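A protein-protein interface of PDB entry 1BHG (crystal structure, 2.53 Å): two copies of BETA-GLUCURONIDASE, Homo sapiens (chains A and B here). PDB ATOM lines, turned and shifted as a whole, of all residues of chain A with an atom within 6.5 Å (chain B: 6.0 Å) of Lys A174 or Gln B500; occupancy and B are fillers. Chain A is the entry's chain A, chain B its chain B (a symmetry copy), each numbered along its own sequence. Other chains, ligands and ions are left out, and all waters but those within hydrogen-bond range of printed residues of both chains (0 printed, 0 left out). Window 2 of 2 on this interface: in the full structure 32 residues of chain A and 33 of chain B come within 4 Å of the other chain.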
ATOM      1  N   LEU A 169     -12.814  22.735 -31.622  1.00  0.00           N
ATOM      2  CA  LEU A 169     -13.011  24.034 -31.000  1.00  0.00           C
ATOM      3  C   LEU A 169     -13.252  23.778 -29.528  1.00  0.00           C
ATOM      4  O   LEU A 169     -14.384  23.561 -29.099  1.00  0.00           O
ATOM      5  CB  LEU A 169     -14.232  24.755 -31.620  1.00  0.00           C
ATOM      6  CG  LEU A 169     -14.356  24.936 -33.151  1.00  0.00           C
ATOM      7  CD1 LEU A 169     -15.793  25.282 -33.517  1.00  0.00           C
ATOM      8  CD2 LEU A 169     -13.376  25.997 -33.679  1.00  0.00           C
ATOM      9  N   THR A 170     -12.162  23.729 -28.773  1.00  0.00           N
ATOM     10  CA  THR A 170     -12.210  23.510 -27.330  1.00  0.00           C
ATOM     11  C   THR A 170     -13.037  24.612 -26.646  1.00  0.00           C
ATOM     12  O   THR A 170     -12.640  25.780 -26.672  1.00  0.00           O
ATOM     13  CB  THR A 170     -10.754  23.466 -26.740  1.00  0.00           C
ATOM     14  OG1 THR A 170      -9.862  24.254 -27.554  1.00  0.00           O
ATOM     15  CG2 THR A 170     -10.270  22.028 -26.677  1.00  0.00           C
ATOM     16  N   ASP A 171     -14.178  24.216 -26.059  1.00  0.00           N
ATOM     17  CA  ASP A 171     -15.117  25.122 -25.358  1.00  0.00           C
ATOM     18  C   ASP A 171     -14.491  26.461 -25.020  1.00  0.00           C
ATOM     19  O   ASP A 171     -13.782  26.596 -24.029  1.00  0.00           O
ATOM     20  CB  ASP A 171     -15.644  24.481 -24.072  1.00  0.00           C
ATOM     21  CG  ASP A 171     -16.940  25.137 -23.559  1.00  0.00           C
ATOM     22  OD1 ASP A 171     -17.110  26.383 -23.673  1.00  0.00           O
ATOM     23  OD2 ASP A 171     -17.794  24.380 -23.016  1.00  0.00           O
ATOM     24  N   THR A 172     -14.736  27.434 -25.879  1.00  0.00           N
ATOM     25  CA  THR A 172     -14.200  28.772 -25.706  1.00  0.00           C
ATOM     26  C   THR A 172     -15.311  29.684 -25.192  1.00  0.00           C
ATOM     27  O   THR A 172     -15.382  30.839 -25.610  1.00  0.00           O
ATOM     28  CB  THR A 172     -13.767  29.316 -27.059  1.00  0.00           C
ATOM     29  OG1 THR A 172     -14.889  29.282 -27.940  1.00  0.00           O
ATOM     30  CG2 THR A 172     -12.719  28.442 -27.677  1.00  0.00           C
ATOM     31  N   SER A 173     -16.190  29.133 -24.337  1.00  0.00           N
ATOM     32  CA  SER A 173     -17.386  29.815 -23.783  1.00  0.00           C
ATOM     33  C   SER A 173     -18.579  29.363 -24.623  1.00  0.00           C
ATOM     34  O   SER A 173     -19.705  29.314 -24.149  1.00  0.00           O
ATOM     35  CB  SER A 173     -17.300  31.357 -23.883  1.00  0.00           C
ATOM     36  OG  SER A 173     -16.486  31.930 -22.861  1.00  0.00           O
ATOM     37  N   LYS A 174     -18.294  29.100 -25.897  1.00  0.00           N
ATOM     38  CA  LYS A 174     -19.222  28.668 -26.938  1.00  0.00           C
ATOM     39  C   LYS A 174     -18.768  27.264 -27.361  1.00  0.00           C
ATOM     40  O   LYS A 174     -17.602  26.927 -27.202  1.00  0.00           O
ATOM     41  CB  LYS A 174     -19.051  29.602 -28.138  1.00  0.00           C
ATOM     42  CG  LYS A 174     -18.887  31.059 -27.776  1.00  0.00           C
ATOM     43  CD  LYS A 174     -18.108  31.795 -28.833  1.00  0.00           C
ATOM     44  CE  LYS A 174     -16.655  31.318 -28.919  1.00  0.00           C
ATOM     45  NZ  LYS A 174     -15.788  32.037 -29.941  1.00  0.00           N
ATOM     46  N   TYR A 175     -19.639  26.508 -28.016  1.00  0.00           N
ATOM     47  CA  TYR A 175     -19.334  25.134 -28.457  1.00  0.00           C
ATOM     48  C   TYR A 175     -19.126  24.179 -27.270  1.00  0.00           C
ATOM     49  O   TYR A 175     -18.318  24.455 -26.377  1.00  0.00           O
ATOM     50  CB  TYR A 175     -18.073  25.057 -29.330  1.00  0.00           C
ATOM     51  CG  TYR A 175     -17.862  26.191 -30.287  1.00  0.00           C
ATOM     52  CD1 TYR A 175     -18.688  26.370 -31.367  1.00  0.00           C
ATOM     53  CD2 TYR A 175     -16.820  27.079 -30.103  1.00  0.00           C
ATOM     54  CE1 TYR A 175     -18.489  27.392 -32.257  1.00  0.00           C
ATOM     55  CE2 TYR A 175     -16.601  28.119 -30.992  1.00  0.00           C
ATOM     56  CZ  TYR A 175     -17.446  28.272 -32.079  1.00  0.00           C
ATOM     57  OH  TYR A 175     -17.192  29.252 -33.034  1.00  0.00           O
ATOM     58  N   PRO A 176     -19.844  23.033 -27.261  1.00  0.00           N
ATOM     59  CA  PRO A 176     -19.780  21.995 -26.226  1.00  0.00           C
ATOM     60  C   PRO A 176     -18.371  21.401 -26.183  1.00  0.00           C
ATOM     61  O   PRO A 176     -17.492  21.796 -26.960  1.00  0.00           O
ATOM     62  CB  PRO A 176     -20.771  20.937 -26.734  1.00  0.00           C
ATOM     63  CG  PRO A 176     -21.721  21.698 -27.596  1.00  0.00           C
ATOM     64  CD  PRO A 176     -20.801  22.656 -28.321  1.00  0.00           C
ATOM     65  N   TYR B 485     -27.178  33.943 -33.067  1.00  0.00           N
ATOM     66  CA  TYR B 485     -26.553  32.604 -33.074  1.00  0.00           C
ATOM     67  C   TYR B 485     -27.258  31.604 -34.039  1.00  0.00           C
ATOM     68  O   TYR B 485     -28.498  31.613 -34.157  1.00  0.00           O
ATOM     69  CB  TYR B 485     -26.543  32.027 -31.660  1.00  0.00           C
ATOM     70  CG  TYR B 485     -25.906  32.930 -30.659  1.00  0.00           C
ATOM     71  CD1 TYR B 485     -24.784  33.708 -31.002  1.00  0.00           C
ATOM     72  CD2 TYR B 485     -26.445  33.065 -29.377  1.00  0.00           C
ATOM     73  CE1 TYR B 485     -24.229  34.596 -30.092  1.00  0.00           C
ATOM     74  CE2 TYR B 485     -25.892  33.939 -28.466  1.00  0.00           C
ATOM     75  CZ  TYR B 485     -24.790  34.701 -28.827  1.00  0.00           C
ATOM     76  OH  TYR B 485     -24.247  35.557 -27.915  1.00  0.00           O
ATOM     77  N   SER B 486     -26.472  30.725 -34.670  1.00  0.00           N
ATOM     78  CA  SER B 486     -26.956  29.730 -35.658  1.00  0.00           C
ATOM     79  C   SER B 486     -27.067  30.405 -37.006  1.00  0.00           C
ATOM     80  O   SER B 486     -26.866  29.771 -38.055  1.00  0.00           O
ATOM     81  CB  SER B 486     -28.315  29.143 -35.301  1.00  0.00           C
ATOM     82  OG  SER B 486     -28.288  28.615 -34.002  1.00  0.00           O
ATOM     83  N   HIS B 489     -23.502  32.929 -37.934  1.00  0.00           N
ATOM     84  CA  HIS B 489     -22.365  32.130 -37.524  1.00  0.00           C
ATOM     85  C   HIS B 489     -22.740  30.769 -37.010  1.00  0.00           C
ATOM     86  O   HIS B 489     -23.707  30.626 -36.272  1.00  0.00           O
ATOM     87  CB  HIS B 489     -21.488  32.839 -36.484  1.00  0.00           C
ATOM     88  CG  HIS B 489     -22.228  33.785 -35.584  1.00  0.00           C
ATOM     89  ND1 HIS B 489     -22.110  35.152 -35.691  1.00  0.00           N
ATOM     90  CD2 HIS B 489     -23.078  33.558 -34.555  1.00  0.00           C
ATOM     91  CE1 HIS B 489     -22.862  35.726 -34.771  1.00  0.00           C
ATOM     92  NE2 HIS B 489     -23.456  34.783 -34.070  1.00  0.00           N
ATOM     93  N   ASP B 490     -21.912  29.790 -37.381  1.00  0.00           N
ATOM     94  CA  ASP B 490     -22.069  28.398 -37.010  1.00  0.00           C
ATOM     95  C   ASP B 490     -23.354  27.957 -37.630  1.00  0.00           C
ATOM     96  O   ASP B 490     -24.163  27.270 -37.009  1.00  0.00           O
ATOM     97  CB  ASP B 490     -22.107  28.240 -35.490  1.00  0.00           C
ATOM     98  CG  ASP B 490     -20.795  28.677 -34.809  1.00  0.00           C
ATOM     99  OD1 ASP B 490     -19.706  28.412 -35.385  1.00  0.00           O
ATOM    100  OD2 ASP B 490     -20.862  29.283 -33.698  1.00  0.00           O
ATOM    101  N   LEU B 496     -26.218  24.985 -30.277  1.00  0.00           N
ATOM    102  CA  LEU B 496     -25.201  25.908 -29.807  1.00  0.00           C
ATOM    103  C   LEU B 496     -25.770  27.148 -29.124  1.00  0.00           C
ATOM    104  O   LEU B 496     -25.136  27.678 -28.206  1.00  0.00           O
ATOM    105  CB  LEU B 496     -24.387  26.342 -30.999  1.00  0.00           C
ATOM    106  CG  LEU B 496     -22.998  25.760 -31.033  1.00  0.00           C
ATOM    107  CD1 LEU B 496     -23.023  24.260 -30.762  1.00  0.00           C
ATOM    108  CD2 LEU B 496     -22.360  26.133 -32.387  1.00  0.00           C
ATOM    109  N   ILE B 497     -26.913  27.641 -29.634  1.00  0.00           N
ATOM    110  CA  ILE B 497     -27.621  28.838 -29.147  1.00  0.00           C
ATOM    111  C   ILE B 497     -27.769  28.946 -27.630  1.00  0.00           C
ATOM    112  O   ILE B 497     -27.187  29.820 -27.011  1.00  0.00           O
ATOM    113  CB  ILE B 497     -29.048  28.943 -29.780  1.00  0.00           C
ATOM    114  CG1 ILE B 497     -28.971  29.221 -31.277  1.00  0.00           C
ATOM    115  CG2 ILE B 497     -29.865  30.041 -29.122  1.00  0.00           C
ATOM    116  CD1 ILE B 497     -30.338  29.176 -31.957  1.00  0.00           C
ATOM    117  N   GLN B 498     -28.573  28.072 -27.052  1.00  0.00           N
ATOM    118  CA  GLN B 498     -28.822  28.065 -25.631  1.00  0.00           C
ATOM    119  C   GLN B 498     -27.664  28.371 -24.730  1.00  0.00           C
ATOM    120  O   GLN B 498     -27.842  28.834 -23.599  1.00  0.00           O
ATOM    121  CB  GLN B 498     -29.416  26.727 -25.219  1.00  0.00           C
ATOM    122  CG  GLN B 498     -30.893  26.572 -25.568  1.00  0.00           C
ATOM    123  CD  GLN B 498     -31.633  25.680 -24.581  1.00  0.00           C
ATOM    124  OE1 GLN B 498     -31.819  26.034 -23.420  1.00  0.00           O
ATOM    125  NE2 GLN B 498     -32.031  24.505 -25.036  1.00  0.00           N
ATOM    126  N   LEU B 499     -26.471  28.047 -25.199  1.00  0.00           N
ATOM    127  CA  LEU B 499     -25.270  28.288 -24.409  1.00  0.00           C
ATOM    128  C   LEU B 499     -24.579  29.589 -24.804  1.00  0.00           C
ATOM    129  O   LEU B 499     -24.410  30.479 -23.956  1.00  0.00           O
ATOM    130  CB  LEU B 499     -24.322  27.086 -24.494  1.00  0.00           C
ATOM    131  CG  LEU B 499     -22.968  27.125 -23.797  1.00  0.00           C
ATOM    132  CD1 LEU B 499     -21.915  27.592 -24.784  1.00  0.00           C
ATOM    133  CD2 LEU B 499     -23.009  27.972 -22.518  1.00  0.00           C
ATOM    134  N   GLN B 500     -24.231  29.737 -26.082  1.00  0.00           N
ATOM    135  CA  GLN B 500     -23.563  30.959 -26.514  1.00  0.00           C
ATOM    136  C   GLN B 500     -24.274  32.198 -25.993  1.00  0.00           C
ATOM    137  O   GLN B 500     -23.674  33.247 -25.854  1.00  0.00           O
ATOM    138  CB  GLN B 500     -23.508  31.030 -28.031  1.00  0.00           C
ATOM    139  CG  GLN B 500     -22.745  29.905 -28.666  1.00  0.00           C
ATOM    140  CD  GLN B 500     -22.664  30.049 -30.174  1.00  0.00           C
ATOM    141  OE1 GLN B 500     -23.594  30.566 -30.825  1.00  0.00           O
ATOM    142  NE2 GLN B 500     -21.544  29.602 -30.745  1.00  0.00           N
ATOM    143  N   LEU B 501     -25.564  32.053 -25.711  1.00  0.00           N
ATOM    144  CA  LEU B 501     -26.431  33.142 -25.228  1.00  0.00           C
ATOM    145  C   LEU B 501     -26.363  33.310 -23.725  1.00  0.00           C
ATOM    146  O   LEU B 501     -26.356  34.410 -23.249  1.00  0.00           O
ATOM    147  CB  LEU B 501     -27.868  32.855 -25.693  1.00  0.00           C
ATOM    148  CG  LEU B 501     -29.019  33.861 -25.750  1.00  0.00           C
ATOM    149  CD1 LEU B 501     -28.774  35.038 -26.743  1.00  0.00           C
ATOM    150  CD2 LEU B 501     -30.248  33.040 -26.142  1.00  0.00           C
ATOM    151  N   ALA B 502     -26.295  32.208 -22.983  1.00  0.00           N
ATOM    152  CA  ALA B 502     -26.187  32.262 -21.515  1.00  0.00           C
ATOM    153  C   ALA B 502     -24.938  33.085 -21.235  1.00  0.00           C
ATOM    154  O   ALA B 502     -24.981  34.149 -20.606  1.00  0.00           O
ATOM    155  CB  ALA B 502     -26.015  30.863 -20.938  1.00  0.00           C
ATOM    156  N   THR B 503     -23.827  32.572 -21.742  1.00  0.00           N
ATOM    157  CA  THR B 503     -22.535  33.216 -21.645  1.00  0.00           C
ATOM    158  C   THR B 503     -22.630  34.727 -21.982  1.00  0.00           C
ATOM    159  O   THR B 503     -22.154  35.539 -21.213  1.00  0.00           O
ATOM    160  CB  THR B 503     -21.548  32.441 -22.576  1.00  0.00           C
ATOM    161  OG1 THR B 503     -21.437  31.093 -22.103  1.00  0.00           O
ATOM    162  CG2 THR B 503     -20.179  33.088 -22.631  1.00  0.00           C
ATOM    163  N   GLN B 504     -23.302  35.102 -23.072  1.00  0.00           N
ATOM    164  CA  GLN B 504     -23.436  36.509 -23.443  1.00  0.00           C
ATOM    165  C   GLN B 504     -24.260  37.311 -22.460  1.00  0.00           C
ATOM    166  O   GLN B 504     -24.211  38.541 -22.474  1.00  0.00           O
ATOM    167  CB  GLN B 504     -23.968  36.710 -24.867  1.00  0.00           C
ATOM    168  CG  GLN B 504     -25.476  36.563 -25.048  1.00  0.00           C
ATOM    169  CD  GLN B 504     -26.100  37.650 -25.914  1.00  0.00           C
ATOM    170  OE1 GLN B 504     -26.528  38.659 -25.407  1.00  0.00           O
ATOM    171  NE2 GLN B 504     -26.185  37.422 -27.205  1.00  0.00           N
ATOM    172  N   PHE B 505     -25.051  36.656 -21.627  1.00  0.00           N
ATOM    173  CA  PHE B 505     -25.764  37.433 -20.639  1.00  0.00           C
ATOM    174  C   PHE B 505     -24.975  37.371 -19.332  1.00  0.00           C
ATOM    175  O   PHE B 505     -25.126  38.248 -18.475  1.00  0.00           O
ATOM    176  CB  PHE B 505     -27.205  36.961 -20.471  1.00  0.00           C
ATOM    177  CG  PHE B 505     -28.145  37.425 -21.582  1.00  0.00           C
ATOM    178  CD1 PHE B 505     -27.878  38.577 -22.325  1.00  0.00           C
ATOM    179  CD2 PHE B 505     -29.312  36.709 -21.863  1.00  0.00           C
ATOM    180  CE1 PHE B 505     -28.745  38.993 -23.328  1.00  0.00           C
ATOM    181  CE2 PHE B 505     -30.181  37.110 -22.853  1.00  0.00           C
ATOM    182  CZ  PHE B 505     -29.902  38.263 -23.591  1.00  0.00           C
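Printed residues of chain B within 4 Å of Ser A173: Leu B499 (2.9 Å) and Thr B503 (3.2 Å).
Of the printed residues of chain B, Tyr A175 touches Asp B490 (3.4 Å) and Leu B496 (3.8 Å).
Of the printed residues of chain A, Leu B496 touches Tyr A175 and Pro A176.
Of chain A, only Lys A174 (3.6 Å) comes within 4 Å of Gln B500.
The nearest residue of chain A that does not touch Gln B500 is Tyr A175 (4.1 Å).
The nearest printed residue of chain B that does not touch Tyr A175 is Gln B500 (4.1 Å).
The side-chain carboxylate (OD1) of Asp A171 is in hydrogen-bond range of the backbone NH (N) of Ser A173, at 3.0 Å.
The backbone carbonyl oxygen (O) of Gln B500 lies within hydrogen-bond range of the side-chain hydroxyl (OH) of Tyr B485.
The side-chain amide nitrogen of Gln B500 is in hydrogen-bond range of the side-chain carboxylate of Asp B490 (3.0 Å).
Of the 14 printed residues of chain B, 5 touch a printed residue of chain A.
Among the printed residues, no Asp or Glu carboxylate lies within 4 Å of a Lys or Arg side-chain nitrogen of the other chain.
Among the printed residues, pairs that only touch across the chains: Ser A173 with Leu B499 (2.9 Å), Tyr A175 with Asp B490 (3.4 Å), Lys A174 with Gln B500 (3.6 Å), Lys A174 with Leu B499 (3.6 Å), Pro A176 with Leu B496 (3.7 Å) and Tyr A175 with Leu B496 (3.8 Å).
The backbone carbonyl oxygen (O) of Ser A173 is in hydrogen-bond range of the side-chain hydroxyl (OG1) of Thr B503.
No position is printed for both chains.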
